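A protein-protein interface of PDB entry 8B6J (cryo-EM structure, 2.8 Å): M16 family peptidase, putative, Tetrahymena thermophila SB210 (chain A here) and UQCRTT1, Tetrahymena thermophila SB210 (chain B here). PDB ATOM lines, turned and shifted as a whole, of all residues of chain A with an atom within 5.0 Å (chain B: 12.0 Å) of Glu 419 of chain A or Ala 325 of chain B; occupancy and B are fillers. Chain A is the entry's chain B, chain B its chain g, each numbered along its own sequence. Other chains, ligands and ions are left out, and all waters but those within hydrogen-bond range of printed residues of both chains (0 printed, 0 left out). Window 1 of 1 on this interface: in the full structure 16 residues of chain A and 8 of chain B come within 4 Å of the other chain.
O of Ser 405 of chain A is in hydrogen-bond range of N of Lys 324 of chain B, at 3.5 Å. O of Ala 328 of chain B lies close to OD1 of Asn 423 of chain A (2.5 Å). The side-chain hydroxyl (OH) of Tyr 435 of chain A sits at hydrogen-bond distance from the chain-end carboxylate (OXT) of Ala 328 of chain B (2.6 Å).
O of Leu 410 of chain A lies within hydrogen-bond range of NH1 of Arg 416 of chain A (2.4 Å). The side-chain carboxylate (OE2) of Glu 419 of chain A sits close to a ring nitrogen (ND1) of His 432 of chain A (3.2 Å). The side-chain hydroxyl of Tyr 435 of chain A sits at hydrogen-bond distance from the side-chain amide oxygen of Asn 423 of chain A (3.1 Å). OE1 of Gln 327 of chain B sits close to O of Ala 325 of chain B.
Among the printed residues, merely in contact across the chains: Ser 405 of chain A with Phe 322 of chain B (3.9 Å), Ser 405 of chain A with Gly 323 of chain B (3.7 Å), Val 406 of chain A with Ala 325 of chain B (3.98 Å), Ala 409 of chain A with Gly 323 of chain B (3.6 Å), Ala 409 of chain A with Lys 324 of chain B (3.4 Å), Ala 409 of chain A with Ala 325 of chain B (3.5 Å), Leu 410 of chain A with Ala 325 of chain B (3.4 Å), Glu 419 of chain A with Ala 325 of chain B (3.7 Å), Glu 419 of chain A with Phe 326 of chain B (3.97 Å), Glu 419 of chain A with Gln 327 of chain B (3.9 Å), Lys 422 of chain A with Gln 327 of chain B (2.9 Å), Lys 422 of chain A with Ala 328 of chain B (3.7 Å) and Tyr 435 of chain A with Phe 326 of chain B (3.5 Å).
Of chain B, only Phe 322, Gly 323 and Lys 324 come within 4 Å of Ser 405 of chain A. Of chain B, only Gly 323, Lys 324 and Ala 325 come within 4 Å of Ala 409 of chain A. Leu 410 of chain A touches one residue of chain B. No residue of chain B comes within 4 Å of Asp 415 of chain A. Arg 416 of chain A touches none of the printed residues of chain B. No residue of chain B comes within 4 Å of Glu 418 of chain A. No residue of chain B comes within 4 Å of Val 421 of chain A. Of chain B, only Ala 328 comes within 4 Å of Asn 423 of chain A. Of the printed residues of chain B, Tyr 435 of chain A touches Phe 326 and Ala 328. Lys 321 of chain B touches none of the printed residues of chain A. Of the printed residues of chain A, Lys 324 of chain B touches Ser 405 (3.5 Å) and Ala 409 (3.4 Å). Of chain A, only Val 406 (3.98 Å), Ala 409 (3.5 Å), Leu 410 (3.4 Å) and Glu 419 (3.7 Å) come within 4 Å of Ala 325 of chain B. Printed residues of chain A within 4 Å of Phe 326 of chain B: Glu 419 (3.97 Å) and Tyr 435 (3.5 Å). Printed residues of chain A within 4 Å of Gln 327 of chain B: Glu 419 (3.9 Å) and Lys 422 (2.9 Å). Of the printed residues of chain A, Ala 328 of chain B touches Lys 422 (3.7 Å), Asn 423 (2.5 Å) and Tyr 435 (2.6 Å). The nearest printed residue of chain B that does not touch Tyr 435 of chain A is Ala 325 of chain B (4.9 Å).
Hydrophobic or aromatic side chains of chain A that line the printed part of chain B: Val 406, Ala 409, Leu 410 and Tyr 435. Hydrophobic or aromatic side chains of chain B within 4 Å of the printed part of chain A: Phe 322, Ala 325 and Phe 326. Among the printed residues, no Asp or Glu carboxylate lies within 4 Å of a Lys or Arg side-chain nitrogen of the other chain.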
ATOM      1  N   SER A 405     -15.398 -29.226 -22.234  1.00  0.00           N
ATOM      2  CA  SER A 405     -14.554 -28.181 -22.809  1.00  0.00           C
ATOM      3  C   SER A 405     -13.104 -28.642 -22.919  1.00  0.00           C
ATOM      4  O   SER A 405     -12.464 -28.486 -23.970  1.00  0.00           O
ATOM      5  CB  SER A 405     -14.650 -26.910 -21.966  1.00  0.00           C
ATOM      6  OG  SER A 405     -15.980 -26.428 -21.920  1.00  0.00           O
ATOM      7  N   VAL A 406     -12.568 -29.220 -21.842  1.00  0.00           N
ATOM      8  CA  VAL A 406     -11.163 -29.614 -21.835  1.00  0.00           C
ATOM      9  C   VAL A 406     -10.905 -30.680 -22.890  1.00  0.00           C
ATOM     10  O   VAL A 406      -9.914 -30.616 -23.626  1.00  0.00           O
ATOM     11  CB  VAL A 406     -10.749 -30.095 -20.432  1.00  0.00           C
ATOM     12  CG1 VAL A 406      -9.343 -30.669 -20.462  1.00  0.00           C
ATOM     13  CG2 VAL A 406     -10.835 -28.954 -19.435  1.00  0.00           C
ATOM     14  N   ALA A 409     -10.919 -29.325 -26.367  1.00  0.00           N
ATOM     15  CA  ALA A 409      -9.622 -28.719 -26.651  1.00  0.00           C
ATOM     16  C   ALA A 409      -8.570 -29.781 -26.951  1.00  0.00           C
ATOM     17  O   ALA A 409      -7.775 -29.631 -27.886  1.00  0.00           O
ATOM     18  CB  ALA A 409      -9.180 -27.853 -25.476  1.00  0.00           C
ATOM     19  N   LEU A 410      -8.551 -30.863 -26.170  1.00  0.00           N
ATOM     20  CA  LEU A 410      -7.493 -31.859 -26.316  1.00  0.00           C
ATOM     21  C   LEU A 410      -7.655 -32.680 -27.587  1.00  0.00           C
ATOM     22  O   LEU A 410      -6.663 -33.177 -28.129  1.00  0.00           O
ATOM     23  CB  LEU A 410      -7.464 -32.797 -25.109  1.00  0.00           C
ATOM     24  CG  LEU A 410      -7.325 -32.199 -23.707  1.00  0.00           C
ATOM     25  CD1 LEU A 410      -6.480 -33.113 -22.831  1.00  0.00           C
ATOM     26  CD2 LEU A 410      -6.758 -30.790 -23.734  1.00  0.00           C
ATOM     27  N   ASP A 415      -3.837 -27.874 -30.175  1.00  0.00           N
ATOM     28  CA  ASP A 415      -4.045 -27.451 -28.795  1.00  0.00           C
ATOM     29  C   ASP A 415      -3.488 -28.480 -27.819  1.00  0.00           C
ATOM     30  O   ASP A 415      -2.938 -28.118 -26.771  1.00  0.00           O
ATOM     31  CB  ASP A 415      -5.533 -27.212 -28.543  1.00  0.00           C
ATOM     32  CG  ASP A 415      -5.791 -26.399 -27.289  1.00  0.00           C
ATOM     33  OD1 ASP A 415      -5.017 -26.533 -26.317  1.00  0.00           O
ATOM     34  OD2 ASP A 415      -6.769 -25.622 -27.274  1.00  0.00           O
ATOM     35  N   ARG A 416      -3.623 -29.766 -28.148  1.00  0.00           N
ATOM     36  CA  ARG A 416      -3.046 -30.801 -27.298  1.00  0.00           C
ATOM     37  C   ARG A 416      -1.538 -30.636 -27.194  1.00  0.00           C
ATOM     38  O   ARG A 416      -0.968 -30.744 -26.104  1.00  0.00           O
ATOM     39  CB  ARG A 416      -3.398 -32.187 -27.839  1.00  0.00           C
ATOM     40  CG  ARG A 416      -2.786 -33.321 -27.035  1.00  0.00           C
ATOM     41  CD  ARG A 416      -3.415 -34.667 -27.357  1.00  0.00           C
ATOM     42  NE  ARG A 416      -3.145 -35.103 -28.723  1.00  0.00           N
ATOM     43  CZ  ARG A 416      -3.984 -34.972 -29.742  1.00  0.00           C
ATOM     44  NH1 ARG A 416      -5.169 -34.401 -29.598  1.00  0.00           N
ATOM     45  NH2 ARG A 416      -3.626 -35.428 -30.938  1.00  0.00           N
ATOM     46  N   LEU A 417      -0.875 -30.359 -28.319  1.00  0.00           N
ATOM     47  CA  LEU A 417       0.570 -30.157 -28.298  1.00  0.00           C
ATOM     48  C   LEU A 417       0.943 -28.924 -27.485  1.00  0.00           C
ATOM     49  O   LEU A 417       1.917 -28.944 -26.722  1.00  0.00           O
ATOM     50  CB  LEU A 417       1.094 -30.035 -29.728  1.00  0.00           C
ATOM     51  CG  LEU A 417       2.599 -29.834 -29.899  1.00  0.00           C
ATOM     52  CD1 LEU A 417       3.374 -30.959 -29.232  1.00  0.00           C
ATOM     53  CD2 LEU A 417       2.941 -29.738 -31.374  1.00  0.00           C
ATOM     54  N   GLU A 418       0.190 -27.835 -27.645  1.00  0.00           N
ATOM     55  CA  GLU A 418       0.490 -26.622 -26.888  1.00  0.00           C
ATOM     56  C   GLU A 418       0.386 -26.878 -25.389  1.00  0.00           C
ATOM     57  O   GLU A 418       1.274 -26.498 -24.612  1.00  0.00           O
ATOM     58  CB  GLU A 418      -0.453 -25.494 -27.309  1.00  0.00           C
ATOM     59  N   GLU A 419      -0.694 -27.534 -24.962  1.00  0.00           N
ATOM     60  CA  GLU A 419      -0.832 -27.823 -23.541  1.00  0.00           C
ATOM     61  C   GLU A 419       0.209 -28.830 -23.076  1.00  0.00           C
ATOM     62  O   GLU A 419       0.613 -28.796 -21.914  1.00  0.00           O
ATOM     63  CB  GLU A 419      -2.237 -28.327 -23.221  1.00  0.00           C
ATOM     64  CG  GLU A 419      -2.582 -29.668 -23.828  1.00  0.00           C
ATOM     65  CD  GLU A 419      -3.693 -30.363 -23.080  1.00  0.00           C
ATOM     66  OE1 GLU A 419      -4.294 -29.735 -22.184  1.00  0.00           O
ATOM     67  OE2 GLU A 419      -3.964 -31.543 -23.387  1.00  0.00           O
ATOM     68  N   THR A 420       0.655 -29.729 -23.955  1.00  0.00           N
ATOM     69  CA  THR A 420       1.738 -30.639 -23.590  1.00  0.00           C
ATOM     70  C   THR A 420       3.016 -29.865 -23.301  1.00  0.00           C
ATOM     71  O   THR A 420       3.707 -30.124 -22.309  1.00  0.00           O
ATOM     72  CB  THR A 420       1.970 -31.653 -24.709  1.00  0.00           C
ATOM     73  OG1 THR A 420       0.866 -32.564 -24.770  1.00  0.00           O
ATOM     74  CG2 THR A 420       3.251 -32.433 -24.471  1.00  0.00           C
ATOM     75  N   VAL A 421       3.343 -28.903 -24.165  1.00  0.00           N
ATOM     76  CA  VAL A 421       4.530 -28.083 -23.939  1.00  0.00           C
ATOM     77  C   VAL A 421       4.408 -27.345 -22.616  1.00  0.00           C
ATOM     78  O   VAL A 421       5.352 -27.296 -21.818  1.00  0.00           O
ATOM     79  CB  VAL A 421       4.739 -27.095 -25.097  1.00  0.00           C
ATOM     80  CG1 VAL A 421       6.018 -26.303 -24.882  1.00  0.00           C
ATOM     81  CG2 VAL A 421       4.781 -27.816 -26.409  1.00  0.00           C
ATOM     82  N   LYS A 422       3.244 -26.742 -22.372  1.00  0.00           N
ATOM     83  CA  LYS A 422       3.077 -25.961 -21.151  1.00  0.00           C
ATOM     84  C   LYS A 422       3.128 -26.852 -19.914  1.00  0.00           C
ATOM     85  O   LYS A 422       3.709 -26.471 -18.891  1.00  0.00           O
ATOM     86  CB  LYS A 422       1.774 -25.169 -21.222  1.00  0.00           C
ATOM     87  CG  LYS A 422       1.761 -24.158 -22.360  1.00  0.00           C
ATOM     88  CD  LYS A 422       0.419 -23.466 -22.501  1.00  0.00           C
ATOM     89  CE  LYS A 422       0.426 -22.464 -23.642  1.00  0.00           C
ATOM     90  NZ  LYS A 422       1.447 -21.403 -23.455  1.00  0.00           N
ATOM     91  N   ASN A 423       2.542 -28.050 -19.987  1.00  0.00           N
ATOM     92  CA  ASN A 423       2.633 -28.985 -18.871  1.00  0.00           C
ATOM     93  C   ASN A 423       4.079 -29.365 -18.595  1.00  0.00           C
ATOM     94  O   ASN A 423       4.509 -29.399 -17.438  1.00  0.00           O
ATOM     95  CB  ASN A 423       1.811 -30.241 -19.162  1.00  0.00           C
ATOM     96  CG  ASN A 423       0.320 -29.979 -19.161  1.00  0.00           C
ATOM     97  OD1 ASN A 423      -0.275 -29.711 -18.120  1.00  0.00           O
ATOM     98  ND2 ASN A 423      -0.296 -30.076 -20.331  1.00  0.00           N
ATOM     99  N   VAL A 424       4.848 -29.660 -19.645  1.00  0.00           N
ATOM    100  CA  VAL A 424       6.243 -30.036 -19.440  1.00  0.00           C
ATOM    101  C   VAL A 424       7.020 -28.880 -18.824  1.00  0.00           C
ATOM    102  O   VAL A 424       7.829 -29.075 -17.910  1.00  0.00           O
ATOM    103  CB  VAL A 424       6.873 -30.505 -20.763  1.00  0.00           C
ATOM    104  CG1 VAL A 424       8.378 -30.647 -20.610  1.00  0.00           C
ATOM    105  CG2 VAL A 424       6.257 -31.824 -21.196  1.00  0.00           C
ATOM    106  N   HIS A 432      -1.887 -33.650 -18.777  1.00  0.00           N
ATOM    107  CA  HIS A 432      -3.139 -33.554 -19.516  1.00  0.00           C
ATOM    108  C   HIS A 432      -3.726 -34.920 -19.836  1.00  0.00           C
ATOM    109  O   HIS A 432      -4.881 -34.993 -20.266  1.00  0.00           O
ATOM    110  CB  HIS A 432      -2.935 -32.753 -20.804  1.00  0.00           C
ATOM    111  CG  HIS A 432      -2.279 -33.525 -21.905  1.00  0.00           C
ATOM    112  ND1 HIS A 432      -2.954 -34.452 -22.671  1.00  0.00           N
ATOM    113  CD2 HIS A 432      -1.012 -33.499 -22.380  1.00  0.00           C
ATOM    114  CE1 HIS A 432      -2.128 -34.969 -23.563  1.00  0.00           C
ATOM    115  NE2 HIS A 432      -0.943 -34.406 -23.408  1.00  0.00           N
ATOM    116  N   TYR A 435      -6.424 -35.384 -16.871  1.00  0.00           N
ATOM    117  CA  TYR A 435      -7.268 -34.263 -16.467  1.00  0.00           C
ATOM    118  C   TYR A 435      -8.637 -34.746 -16.005  1.00  0.00           C
ATOM    119  O   TYR A 435      -9.202 -34.204 -15.048  1.00  0.00           O
ATOM    120  CB  TYR A 435      -7.421 -33.269 -17.621  1.00  0.00           C
ATOM    121  CG  TYR A 435      -6.320 -32.229 -17.754  1.00  0.00           C
ATOM    122  CD1 TYR A 435      -5.491 -31.901 -16.686  1.00  0.00           C
ATOM    123  CD2 TYR A 435      -6.127 -31.560 -18.955  1.00  0.00           C
ATOM    124  CE1 TYR A 435      -4.500 -30.951 -16.816  1.00  0.00           C
ATOM    125  CE2 TYR A 435      -5.137 -30.606 -19.092  1.00  0.00           C
ATOM    126  CZ  TYR A 435      -4.328 -30.306 -18.020  1.00  0.00           C
ATOM    127  OH  TYR A 435      -3.341 -29.357 -18.153  1.00  0.00           O
ATOM    128  N   PRO B 320     -12.531 -17.831 -31.894  1.00  0.00           N
ATOM    129  CA  PRO B 320     -11.781 -19.029 -31.507  1.00  0.00           C
ATOM    130  C   PRO B 320     -12.686 -20.241 -31.363  1.00  0.00           C
ATOM    131  O   PRO B 320     -13.886 -20.127 -31.104  1.00  0.00           O
ATOM    132  CB  PRO B 320     -11.155 -18.638 -30.163  1.00  0.00           C
ATOM    133  CG  PRO B 320     -12.035 -17.566 -29.634  1.00  0.00           C
ATOM    134  CD  PRO B 320     -12.526 -16.811 -30.831  1.00  0.00           C
ATOM    135  N   LYS B 321     -12.090 -21.417 -31.538  1.00  0.00           N
ATOM    136  CA  LYS B 321     -12.844 -22.657 -31.459  1.00  0.00           C
ATOM    137  C   LYS B 321     -13.409 -22.850 -30.052  1.00  0.00           C
ATOM    138  O   LYS B 321     -13.105 -22.109 -29.116  1.00  0.00           O
ATOM    139  CB  LYS B 321     -11.961 -23.840 -31.848  1.00  0.00           C
ATOM    140  CG  LYS B 321     -11.452 -23.776 -33.276  1.00  0.00           C
ATOM    141  CD  LYS B 321     -10.654 -25.012 -33.643  1.00  0.00           C
ATOM    142  CE  LYS B 321     -10.165 -24.949 -35.079  1.00  0.00           C
ATOM    143  NZ  LYS B 321      -9.433 -26.183 -35.476  1.00  0.00           N
ATOM    144  N   PHE B 322     -14.254 -23.874 -29.918  1.00  0.00           N
ATOM    145  CA  PHE B 322     -14.985 -24.078 -28.672  1.00  0.00           C
ATOM    146  C   PHE B 322     -14.069 -24.534 -27.542  1.00  0.00           C
ATOM    147  O   PHE B 322     -14.195 -24.059 -26.407  1.00  0.00           O
ATOM    148  CB  PHE B 322     -16.105 -25.095 -28.891  1.00  0.00           C
ATOM    149  CG  PHE B 322     -16.766 -25.549 -27.625  1.00  0.00           C
ATOM    150  CD1 PHE B 322     -17.740 -24.775 -27.022  1.00  0.00           C
ATOM    151  CD2 PHE B 322     -16.418 -26.753 -27.040  1.00  0.00           C
ATOM    152  CE1 PHE B 322     -18.351 -25.191 -25.856  1.00  0.00           C
ATOM    153  CE2 PHE B 322     -17.025 -27.173 -25.875  1.00  0.00           C
ATOM    154  CZ  PHE B 322     -17.992 -26.392 -25.284  1.00  0.00           C
ATOM    155  N   GLY B 323     -13.147 -25.448 -27.827  1.00  0.00           N
ATOM    156  CA  GLY B 323     -12.373 -26.058 -26.762  1.00  0.00           C
ATOM    157  C   GLY B 323     -11.527 -25.047 -26.012  1.00  0.00           C
ATOM    158  O   GLY B 323     -11.045 -24.061 -26.572  1.00  0.00           O
ATOM    159  N   LYS B 324     -11.351 -25.304 -24.715  1.00  0.00           N
ATOM    160  CA  LYS B 324     -10.482 -24.477 -23.881  1.00  0.00           C
ATOM    161  C   LYS B 324     -10.026 -25.331 -22.705  1.00  0.00           C
ATOM    162  O   LYS B 324     -10.823 -25.613 -21.805  1.00  0.00           O
ATOM    163  CB  LYS B 324     -11.215 -23.228 -23.407  1.00  0.00           C
ATOM    164  CG  LYS B 324     -10.305 -22.123 -22.897  1.00  0.00           C
ATOM    165  CD  LYS B 324      -9.555 -21.456 -24.037  1.00  0.00           C
ATOM    166  CE  LYS B 324      -8.771 -20.247 -23.559  1.00  0.00           C
ATOM    167  NZ  LYS B 324      -8.093 -19.545 -24.684  1.00  0.00           N
ATOM    168  N   ALA B 325      -8.760 -25.732 -22.711  1.00  0.00           N
ATOM    169  CA  ALA B 325      -8.207 -26.602 -21.684  1.00  0.00           C
ATOM    170  C   ALA B 325      -7.329 -25.810 -20.722  1.00  0.00           C
ATOM    171  O   ALA B 325      -6.997 -24.646 -20.951  1.00  0.00           O
ATOM    172  CB  ALA B 325      -7.400 -27.736 -22.319  1.00  0.00           C
ATOM    173  N   PHE B 326      -6.955 -26.465 -19.624  1.00  0.00           N
ATOM    174  CA  PHE B 326      -6.007 -25.871 -18.692  1.00  0.00           C
ATOM    175  C   PHE B 326      -4.725 -25.533 -19.437  1.00  0.00           C
ATOM    176  O   PHE B 326      -4.084 -26.416 -20.014  1.00  0.00           O
ATOM    177  CB  PHE B 326      -5.715 -26.833 -17.541  1.00  0.00           C
ATOM    178  CG  PHE B 326      -6.940 -27.317 -16.817  1.00  0.00           C
ATOM    179  CD1 PHE B 326      -8.105 -26.570 -16.808  1.00  0.00           C
ATOM    180  CD2 PHE B 326      -6.923 -28.524 -16.140  1.00  0.00           C
ATOM    181  CE1 PHE B 326      -9.226 -27.020 -16.140  1.00  0.00           C
ATOM    182  CE2 PHE B 326      -8.040 -28.977 -15.473  1.00  0.00           C
ATOM    183  CZ  PHE B 326      -9.193 -28.225 -15.472  1.00  0.00           C
ATOM    184  N   GLN B 327      -4.350 -24.254 -19.426  1.00  0.00           N
ATOM    185  CA  GLN B 327      -3.242 -23.810 -20.264  1.00  0.00           C
ATOM    186  C   GLN B 327      -1.964 -24.568 -19.929  1.00  0.00           C
ATOM    187  O   GLN B 327      -1.288 -25.092 -20.820  1.00  0.00           O
ATOM    188  CB  GLN B 327      -3.037 -22.303 -20.105  1.00  0.00           C
ATOM    189  CG  GLN B 327      -2.684 -21.588 -21.400  1.00  0.00           C
ATOM    190  CD  GLN B 327      -3.822 -21.601 -22.405  1.00  0.00           C
ATOM    191  OE1 GLN B 327      -4.854 -22.235 -22.185  1.00  0.00           O
ATOM    192  NE2 GLN B 327      -3.639 -20.895 -23.515  1.00  0.00           N
ATOM    193  N   ALA B 328      -1.627 -24.655 -18.648  1.00  0.00           N
ATOM    194  CA  ALA B 328      -0.420 -25.358 -18.228  1.00  0.00           C
ATOM    195  C   ALA B 328      -0.758 -26.762 -17.748  1.00  0.00           C
ATOM    196  O   ALA B 328       0.051 -27.410 -17.085  1.00  0.00           O
ATOM    197  CB  ALA B 328       0.290 -24.583 -17.137  1.00  0.00           C
ATOM    198  OXT ALA B 328      -1.843 -27.279 -18.009  1.00  0.00           O
